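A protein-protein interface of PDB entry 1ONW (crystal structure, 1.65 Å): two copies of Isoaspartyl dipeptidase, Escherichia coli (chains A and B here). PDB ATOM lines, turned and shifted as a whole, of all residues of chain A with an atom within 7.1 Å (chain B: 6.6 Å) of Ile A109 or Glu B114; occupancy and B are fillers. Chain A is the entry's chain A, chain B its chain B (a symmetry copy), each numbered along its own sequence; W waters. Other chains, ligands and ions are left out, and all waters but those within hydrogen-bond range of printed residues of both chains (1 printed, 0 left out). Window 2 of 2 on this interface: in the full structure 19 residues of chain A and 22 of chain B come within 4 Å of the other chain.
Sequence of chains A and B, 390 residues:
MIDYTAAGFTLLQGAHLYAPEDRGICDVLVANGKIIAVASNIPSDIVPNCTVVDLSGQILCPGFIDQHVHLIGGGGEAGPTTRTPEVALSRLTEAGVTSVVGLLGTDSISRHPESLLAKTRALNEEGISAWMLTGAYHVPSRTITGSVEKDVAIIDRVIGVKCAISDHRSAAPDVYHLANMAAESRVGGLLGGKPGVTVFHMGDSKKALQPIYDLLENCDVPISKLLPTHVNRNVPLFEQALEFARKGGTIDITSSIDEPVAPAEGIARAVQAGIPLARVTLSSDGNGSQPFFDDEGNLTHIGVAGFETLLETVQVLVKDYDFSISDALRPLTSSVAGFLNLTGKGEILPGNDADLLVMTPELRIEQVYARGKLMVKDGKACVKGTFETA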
ATOM      1  N   ARG A  83      -6.682 -23.269 -17.926  1.00  0.00           N
ATOM      2  CA  ARG A  83      -7.021 -22.292 -18.962  1.00  0.00           C
ATOM      3  C   ARG A  83      -8.369 -22.665 -19.520  1.00  0.00           C
ATOM      4  O   ARG A  83      -8.552 -23.788 -20.004  1.00  0.00           O
ATOM      5  CB  ARG A  83      -6.009 -22.341 -20.085  1.00  0.00           C
ATOM      6  CG  ARG A  83      -4.636 -21.938 -19.559  1.00  0.00           C
ATOM      7  CD  ARG A  83      -3.522 -22.163 -20.583  1.00  0.00           C
ATOM      8  NE  ARG A  83      -3.576 -21.262 -21.738  1.00  0.00           N
ATOM      9  CZ  ARG A  83      -3.996 -21.631 -22.946  1.00  0.00           C
ATOM     10  NH1 ARG A  83      -4.426 -22.853 -23.224  1.00  0.00           N
ATOM     11  NH2 ARG A  83      -3.991 -20.721 -23.915  1.00  0.00           N
ATOM     12  N   LEU A 104      -9.257  -9.724 -21.159  1.00  0.00           N
ATOM     13  CA  LEU A 104      -8.272 -10.675 -20.635  1.00  0.00           C
ATOM     14  C   LEU A 104      -8.116 -10.427 -19.129  1.00  0.00           C
ATOM     15  O   LEU A 104      -8.503  -9.369 -18.629  1.00  0.00           O
ATOM     16  CB  LEU A 104      -6.878 -10.502 -21.300  1.00  0.00           C
ATOM     17  CG  LEU A 104      -6.847 -10.635 -22.830  1.00  0.00           C
ATOM     18  CD1 LEU A 104      -5.388 -10.523 -23.298  1.00  0.00           C
ATOM     19  CD2 LEU A 104      -7.368 -12.025 -23.225  1.00  0.00           C
ATOM     20  N   THR A 106      -5.769 -12.352 -15.551  1.00  0.00           N
ATOM     21  CA  THR A 106      -4.477 -12.654 -14.981  1.00  0.00           C
ATOM     22  C   THR A 106      -3.452 -13.016 -16.045  1.00  0.00           C
ATOM     23  O   THR A 106      -2.342 -12.487 -16.074  1.00  0.00           O
ATOM     24  CB  THR A 106      -4.606 -13.812 -13.985  1.00  0.00           C
ATOM     25  OG1 THR A 106      -5.640 -13.482 -13.097  1.00  0.00           O
ATOM     26  CG2 THR A 106      -3.311 -13.923 -13.221  1.00  0.00           C
ATOM     27  N   ASP A 107      -3.831 -13.941 -16.927  1.00  0.00           N
ATOM     28  CA  ASP A 107      -2.902 -14.399 -17.924  1.00  0.00           C
ATOM     29  C   ASP A 107      -2.893 -13.602 -19.190  1.00  0.00           C
ATOM     30  O   ASP A 107      -3.852 -13.586 -19.947  1.00  0.00           O
ATOM     31  CB  ASP A 107      -3.219 -15.867 -18.231  1.00  0.00           C
ATOM     32  CG  ASP A 107      -2.296 -16.529 -19.234  1.00  0.00           C
ATOM     33  OD1 ASP A 107      -1.341 -15.989 -19.759  1.00  0.00           O
ATOM     34  OD2 ASP A 107      -2.637 -17.771 -19.457  1.00  0.00           O
ATOM     35  N   SER A 108      -1.750 -12.966 -19.433  1.00  0.00           N
ATOM     36  CA  SER A 108      -1.530 -12.231 -20.665  1.00  0.00           C
ATOM     37  C   SER A 108      -0.244 -12.742 -21.292  1.00  0.00           C
ATOM     38  O   SER A 108       0.439 -12.058 -22.064  1.00  0.00           O
ATOM     39  CB  SER A 108      -1.663 -10.690 -20.586  1.00  0.00           C
ATOM     40  OG  SER A 108      -0.878 -10.125 -19.553  1.00  0.00           O
ATOM     41  N   ILE A 109       0.079 -13.996 -20.948  1.00  0.00           N
ATOM     42  CA  ILE A 109       1.265 -14.667 -21.484  1.00  0.00           C
ATOM     43  C   ILE A 109       0.867 -15.665 -22.571  1.00  0.00           C
ATOM     44  O   ILE A 109       1.415 -15.727 -23.679  1.00  0.00           O
ATOM     45  CB  ILE A 109       2.065 -15.387 -20.398  1.00  0.00           C
ATOM     46  CG1 ILE A 109       2.607 -14.393 -19.382  1.00  0.00           C
ATOM     47  CG2 ILE A 109       3.247 -16.149 -21.000  1.00  0.00           C
ATOM     48  CD1 ILE A 109       3.776 -13.581 -19.923  1.00  0.00           C
ATOM     49  N   SER A 110      -0.128 -16.442 -22.241  1.00  0.00           N
ATOM     50  CA  SER A 110      -0.637 -17.414 -23.177  1.00  0.00           C
ATOM     51  C   SER A 110      -1.935 -16.892 -23.797  1.00  0.00           C
ATOM     52  O   SER A 110      -2.543 -17.578 -24.605  1.00  0.00           O
ATOM     53  CB  SER A 110      -0.915 -18.710 -22.458  1.00  0.00           C
ATOM     54  OG  SER A 110      -2.229 -18.650 -21.904  1.00  0.00           O
ATOM     55  N   ARG A 111      -2.378 -15.678 -23.389  1.00  0.00           N
ATOM     56  CA  ARG A 111      -3.585 -15.029 -23.934  1.00  0.00           C
ATOM     57  C   ARG A 111      -3.121 -13.738 -24.579  1.00  0.00           C
ATOM     58  O   ARG A 111      -2.307 -13.041 -23.997  1.00  0.00           O
ATOM     59  CB  ARG A 111      -4.592 -14.708 -22.844  1.00  0.00           C
ATOM     60  CG  ARG A 111      -5.053 -15.952 -22.062  1.00  0.00           C
ATOM     61  CD  ARG A 111      -5.665 -17.062 -22.917  1.00  0.00           C
ATOM     62  NE  ARG A 111      -6.297 -18.082 -22.078  1.00  0.00           N
ATOM     63  CZ  ARG A 111      -7.063 -19.080 -22.547  1.00  0.00           C
ATOM     64  NH1 ARG A 111      -7.334 -19.189 -23.841  1.00  0.00           N
ATOM     65  NH2 ARG A 111      -7.627 -19.949 -21.687  1.00  0.00           N
ATOM     66  N   HIS A 112      -3.627 -13.408 -25.777  1.00  0.00           N
ATOM     67  CA  HIS A 112      -3.172 -12.241 -26.542  1.00  0.00           C
ATOM     68  C   HIS A 112      -4.291 -11.336 -27.046  1.00  0.00           C
ATOM     69  O   HIS A 112      -5.343 -11.829 -27.401  1.00  0.00           O
ATOM     70  CB  HIS A 112      -2.330 -12.750 -27.744  1.00  0.00           C
ATOM     71  CG  HIS A 112      -1.169 -13.590 -27.311  1.00  0.00           C
ATOM     72  ND1 HIS A 112      -1.345 -14.938 -27.000  1.00  0.00           N
ATOM     73  CD2 HIS A 112       0.147 -13.280 -27.118  1.00  0.00           C
ATOM     74  CE1 HIS A 112      -0.162 -15.408 -26.592  1.00  0.00           C
ATOM     75  NE2 HIS A 112       0.762 -14.443 -26.659  1.00  0.00           N
ATOM     76  N   ALA A 136      -4.745  -6.252 -19.919  1.00  0.00           N
ATOM     77  CA  ALA A 136      -5.127  -7.416 -19.130  1.00  0.00           C
ATOM     78  C   ALA A 136      -4.822  -7.025 -17.692  1.00  0.00           C
ATOM     79  O   ALA A 136      -4.645  -5.842 -17.420  1.00  0.00           O
ATOM     80  CB  ALA A 136      -4.289  -8.634 -19.545  1.00  0.00           C
ATOM     81  N   ARG A 142      -0.155  -4.799 -22.048  1.00  0.00           N
ATOM     82  CA  ARG A 142       0.334  -5.510 -23.219  1.00  0.00           C
ATOM     83  C   ARG A 142      -0.681  -5.245 -24.319  1.00  0.00           C
ATOM     84  O   ARG A 142      -1.839  -5.565 -24.158  1.00  0.00           O
ATOM     85  CB  ARG A 142       0.448  -6.969 -22.862  1.00  0.00           C
ATOM     86  CG  ARG A 142       1.548  -7.114 -21.819  1.00  0.00           C
ATOM     87  CD  ARG A 142       1.637  -8.532 -21.318  1.00  0.00           C
ATOM     88  NE  ARG A 142       2.828  -8.756 -20.517  1.00  0.00           N
ATOM     89  CZ  ARG A 142       2.864  -9.539 -19.451  1.00  0.00           C
ATOM     90  NH1 ARG A 142       1.778 -10.195 -19.026  1.00  0.00           N
ATOM     91  NH2 ARG A 142       4.027  -9.661 -18.805  1.00  0.00           N
ATOM     92  N   HIS B 112      -0.337 -17.956 -31.281  1.00  0.00           N
ATOM     93  CA  HIS B 112       0.994 -17.690 -30.781  1.00  0.00           C
ATOM     94  C   HIS B 112       1.676 -18.910 -30.181  1.00  0.00           C
ATOM     95  O   HIS B 112       1.038 -19.754 -29.576  1.00  0.00           O
ATOM     96  CB  HIS B 112       0.878 -16.601 -29.689  1.00  0.00           C
ATOM     97  CG  HIS B 112       0.076 -15.415 -30.166  1.00  0.00           C
ATOM     98  ND1 HIS B 112      -1.319 -15.422 -30.210  1.00  0.00           N
ATOM     99  CD2 HIS B 112       0.500 -14.215 -30.654  1.00  0.00           C
ATOM    100  CE1 HIS B 112      -1.715 -14.234 -30.696  1.00  0.00           C
ATOM    101  NE2 HIS B 112      -0.642 -13.496 -30.998  1.00  0.00           N
ATOM    102  N   PRO B 113       2.989 -18.997 -30.327  1.00  0.00           N
ATOM    103  CA  PRO B 113       3.711 -20.139 -29.778  1.00  0.00           C
ATOM    104  C   PRO B 113       3.550 -20.290 -28.277  1.00  0.00           C
ATOM    105  O   PRO B 113       3.569 -21.387 -27.772  1.00  0.00           O
ATOM    106  CB  PRO B 113       5.181 -19.988 -30.180  1.00  0.00           C
ATOM    107  CG  PRO B 113       5.334 -18.589 -30.741  1.00  0.00           C
ATOM    108  CD  PRO B 113       3.925 -18.121 -31.092  1.00  0.00           C
ATOM    109  N   GLU B 114       3.414 -19.188 -27.559  1.00  0.00           N
ATOM    110  CA  GLU B 114       3.242 -19.202 -26.124  1.00  0.00           C
ATOM    111  C   GLU B 114       1.940 -19.877 -25.753  1.00  0.00           C
ATOM    112  O   GLU B 114       1.849 -20.569 -24.723  1.00  0.00           O
ATOM    113  CB  GLU B 114       3.253 -17.780 -25.560  1.00  0.00           C
ATOM    114  CG  GLU B 114       4.653 -17.101 -25.694  1.00  0.00           C
ATOM    115  CD  GLU B 114       4.849 -16.356 -26.974  1.00  0.00           C
ATOM    116  OE1 GLU B 114       4.124 -16.458 -27.918  1.00  0.00           O
ATOM    117  OE2 GLU B 114       5.903 -15.613 -26.985  1.00  0.00           O
ATOM    118  N   SER B 115       0.931 -19.654 -26.584  1.00  0.00           N
ATOM    119  CA  SER B 115      -0.344 -20.280 -26.343  1.00  0.00           C
ATOM    120  C   SER B 115      -0.213 -21.769 -26.516  1.00  0.00           C
ATOM    121  O   SER B 115      -0.647 -22.570 -25.686  1.00  0.00           O
ATOM    122  CB  SER B 115      -1.393 -19.761 -27.286  1.00  0.00           C
ATOM    123  OG  SER B 115      -1.570 -18.371 -27.056  1.00  0.00           O
ATOM    124  N   LEU B 116       0.387 -22.130 -27.648  1.00  0.00           N
ATOM    125  CA  LEU B 116       0.610 -23.529 -27.947  1.00  0.00           C
ATOM    126  C   LEU B 116       1.406 -24.253 -26.853  1.00  0.00           C
ATOM    127  O   LEU B 116       1.110 -25.402 -26.504  1.00  0.00           O
ATOM    128  CB  LEU B 116       1.215 -23.675 -29.379  1.00  0.00           C
ATOM    129  CG  LEU B 116       1.575 -25.081 -29.824  1.00  0.00           C
ATOM    130  CD1 LEU B 116       0.339 -25.946 -29.929  1.00  0.00           C
ATOM    131  CD2 LEU B 116       2.250 -25.008 -31.183  1.00  0.00           C
ATOM    132  N   LEU B 117       2.449 -23.600 -26.307  1.00  0.00           N
ATOM    133  CA  LEU B 117       3.265 -24.197 -25.280  1.00  0.00           C
ATOM    134  C   LEU B 117       2.451 -24.473 -24.035  1.00  0.00           C
ATOM    135  O   LEU B 117       2.649 -25.491 -23.389  1.00  0.00           O
ATOM    136  CB  LEU B 117       4.390 -23.200 -24.921  1.00  0.00           C
ATOM    137  CG  LEU B 117       5.317 -23.620 -23.795  1.00  0.00           C
ATOM    138  CD1 LEU B 117       6.019 -24.921 -24.154  1.00  0.00           C
ATOM    139  CD2 LEU B 117       6.364 -22.517 -23.569  1.00  0.00           C
ATOM    140  N   ALA B 118       1.537 -23.526 -23.685  1.00  0.00           N
ATOM    141  CA  ALA B 118       0.709 -23.674 -22.493  1.00  0.00           C
ATOM    142  C   ALA B 118      -0.192 -24.901 -22.648  1.00  0.00           C
ATOM    143  O   ALA B 118      -0.336 -25.723 -21.731  1.00  0.00           O
ATOM    144  CB  ALA B 118      -0.098 -22.400 -22.218  1.00  0.00           C
ATOM    145  N   LYS B 119      -0.790 -25.016 -23.850  1.00  0.00           N
ATOM    146  CA  LYS B 119      -1.646 -26.141 -24.201  1.00  0.00           C
ATOM    147  C   LYS B 119      -0.895 -27.470 -24.140  1.00  0.00           C
ATOM    148  O   LYS B 119      -1.393 -28.470 -23.655  1.00  0.00           O
ATOM    149  CB  LYS B 119      -2.338 -25.943 -25.553  1.00  0.00           C
ATOM    150  CG  LYS B 119      -3.258 -27.128 -25.932  1.00  0.00           C
ATOM    151  CD  LYS B 119      -4.502 -27.360 -25.054  1.00  0.00           C
ATOM    152  CE  LYS B 119      -5.486 -28.388 -25.587  1.00  0.00           C
ATOM    153  NZ  LYS B 119      -6.728 -28.545 -24.795  1.00  0.00           N
ATOM    154  N   MET B 132       5.970 -29.607 -29.180  1.00  0.00           N
ATOM    155  CA  MET B 132       5.484 -28.702 -30.208  1.00  0.00           C
ATOM    156  C   MET B 132       6.603 -28.229 -31.124  1.00  0.00           C
ATOM    157  O   MET B 132       7.803 -28.356 -30.826  1.00  0.00           O
ATOM    158  CB  MET B 132       4.877 -27.437 -29.536  1.00  0.00           C
ATOM    159  CG  MET B 132       5.901 -26.660 -28.694  1.00  0.00           C
ATOM    160  SD  MET B 132       5.333 -25.055 -28.046  1.00  0.00           S
ATOM    161  CE  MET B 132       5.560 -23.900 -29.448  1.00  0.00           C
ATOM    162  N   THR B 143       8.715 -16.621 -33.201  1.00  0.00           N
ATOM    163  CA  THR B 143       9.114 -17.479 -32.100  1.00  0.00           C
ATOM    164  C   THR B 143       8.801 -16.908 -30.745  1.00  0.00           C
ATOM    165  O   THR B 143       8.300 -15.815 -30.627  1.00  0.00           O
ATOM    166  CB  THR B 143      10.653 -17.645 -32.162  1.00  0.00           C
ATOM    167  OG1 THR B 143      11.266 -16.376 -31.982  1.00  0.00           O
ATOM    168  CG2 THR B 143      11.056 -18.205 -33.516  1.00  0.00           C
ATOM    169  N   ILE B 144       9.139 -17.688 -29.722  1.00  0.00           N
ATOM    170  CA  ILE B 144       8.934 -17.290 -28.346  1.00  0.00           C
ATOM    171  C   ILE B 144      10.064 -16.419 -27.835  1.00  0.00           C
ATOM    172  O   ILE B 144       9.842 -15.376 -27.200  1.00  0.00           O
ATOM    173  CB  ILE B 144       8.875 -18.544 -27.490  1.00  0.00           C
ATOM    174  CG1 ILE B 144       7.690 -19.376 -27.904  1.00  0.00           C
ATOM    175  CG2 ILE B 144       8.800 -18.184 -26.010  1.00  0.00           C
ATOM    176  CD1 ILE B 144       7.552 -20.643 -27.068  1.00  0.00           C
ATOM    177  N   THR B 145      11.297 -16.874 -28.094  1.00  0.00           N
ATOM    178  CA  THR B 145      12.487 -16.213 -27.597  1.00  0.00           C
ATOM    179  C   THR B 145      13.170 -15.283 -28.552  1.00  0.00           C
ATOM    180  O   THR B 145      14.142 -14.647 -28.160  1.00  0.00           O
ATOM    181  CB  THR B 145      13.551 -17.231 -27.198  1.00  0.00           C
ATOM    182  OG1 THR B 145      14.027 -17.815 -28.400  1.00  0.00           O
ATOM    183  CG2 THR B 145      12.968 -18.227 -26.205  1.00  0.00           C
HETATM  184  O   HOH W   1      -3.953 -15.831 -27.229  1.00  0.00           O
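Water W1 lies within hydrogen-bond range of a ring nitrogen (ND1) of His A112 (2.8 Å), the backbone carbonyl oxygen (O) of Ser A110 (3.5 Å) and the side-chain hydroxyl (OG) of Ser B115 (3.5 Å).
Of the 11 printed residues of chain A, 4 touch a printed residue of chain B. Along chain A the printed residues that touch a printed residue of chain B span positions 83 to 112. Of the 12 printed residues of chain B, 4 touch a printed residue of chain A. Hydrophobic or aromatic side chains of chain B that line the printed part of chain A: His B112 and Ala B118.
Ile A109 touches just one residue of chain B: Glu B114. Glu B114 touches just one residue of chain A: Ile A109 (3.3 Å). Printed residues of chain B within 4 Å of Ser A110: Ser B115 and Ala B118. Of the printed residues of chain A, Ala B118 touches Arg A83 (3.7 Å) and Ser A110 (3.8 Å). Printed residues of chain B within 4 Å of Arg A83: Ala B118. Of the printed residues of chain B, His A112 touches His B112 (3.2 Å) and Ser B115 (3.3 Å). Of the printed residues of chain A, Ser B115 touches Ser A110 (2.8 Å) and His A112 (3.3 Å). The nearest residue of chain B that does not touch Ile A109 is Ser B115 (4.9 Å). The nearest residue of chain A that does not touch Glu B114 is Ser A110 (4.03 Å). The nearest printed residue of chain B that does not touch His A112 is Glu B114 (4.1 Å).
Among the printed residues, merely in contact across the chains: Ile A109 with Glu B114 (3.3 Å), Arg A83 with Ala B118 (3.7 Å) and Ser A110 with Ala B118 (3.8 Å).
A ring nitrogen (ND1) of His A112 lies close to the side-chain hydroxyl (OG) of Ser B115 (3.4 Å). The side-chain hydroxyl (OG) of Ser B115 sits at hydrogen-bond distance from the backbone carbonyl oxygen (O) of Ser A110, at 2.8 Å. ND1 of His A112 lies within hydrogen-bond range of ND1 of His B112 (3.2 Å).
The guanidinium group of Arg A83 lies within hydrogen-bond range of the side-chain hydroxyl of Ser A110, 2.9 Å away. The side-chain carboxylate of Asp A107 sits at hydrogen-bond distance from the side-chain hydroxyl of Ser A110 (2.6 Å). A ring nitrogen (NE2) of His A112 lies within hydrogen-bond range of the backbone carbonyl oxygen (O) of Ile A109, at 3.3 Å. The backbone NH (N) of Ile A109 lies within hydrogen-bond range of the side-chain carboxylate (OD1) of Asp A107 (2.7 Å).
His A112 touches its own counterpart, His B112. 1 position is printed for both chains. Of the 6 pairs that touch across the chains among the printed residues, 1 has its exchanged pair printed and touching as well.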
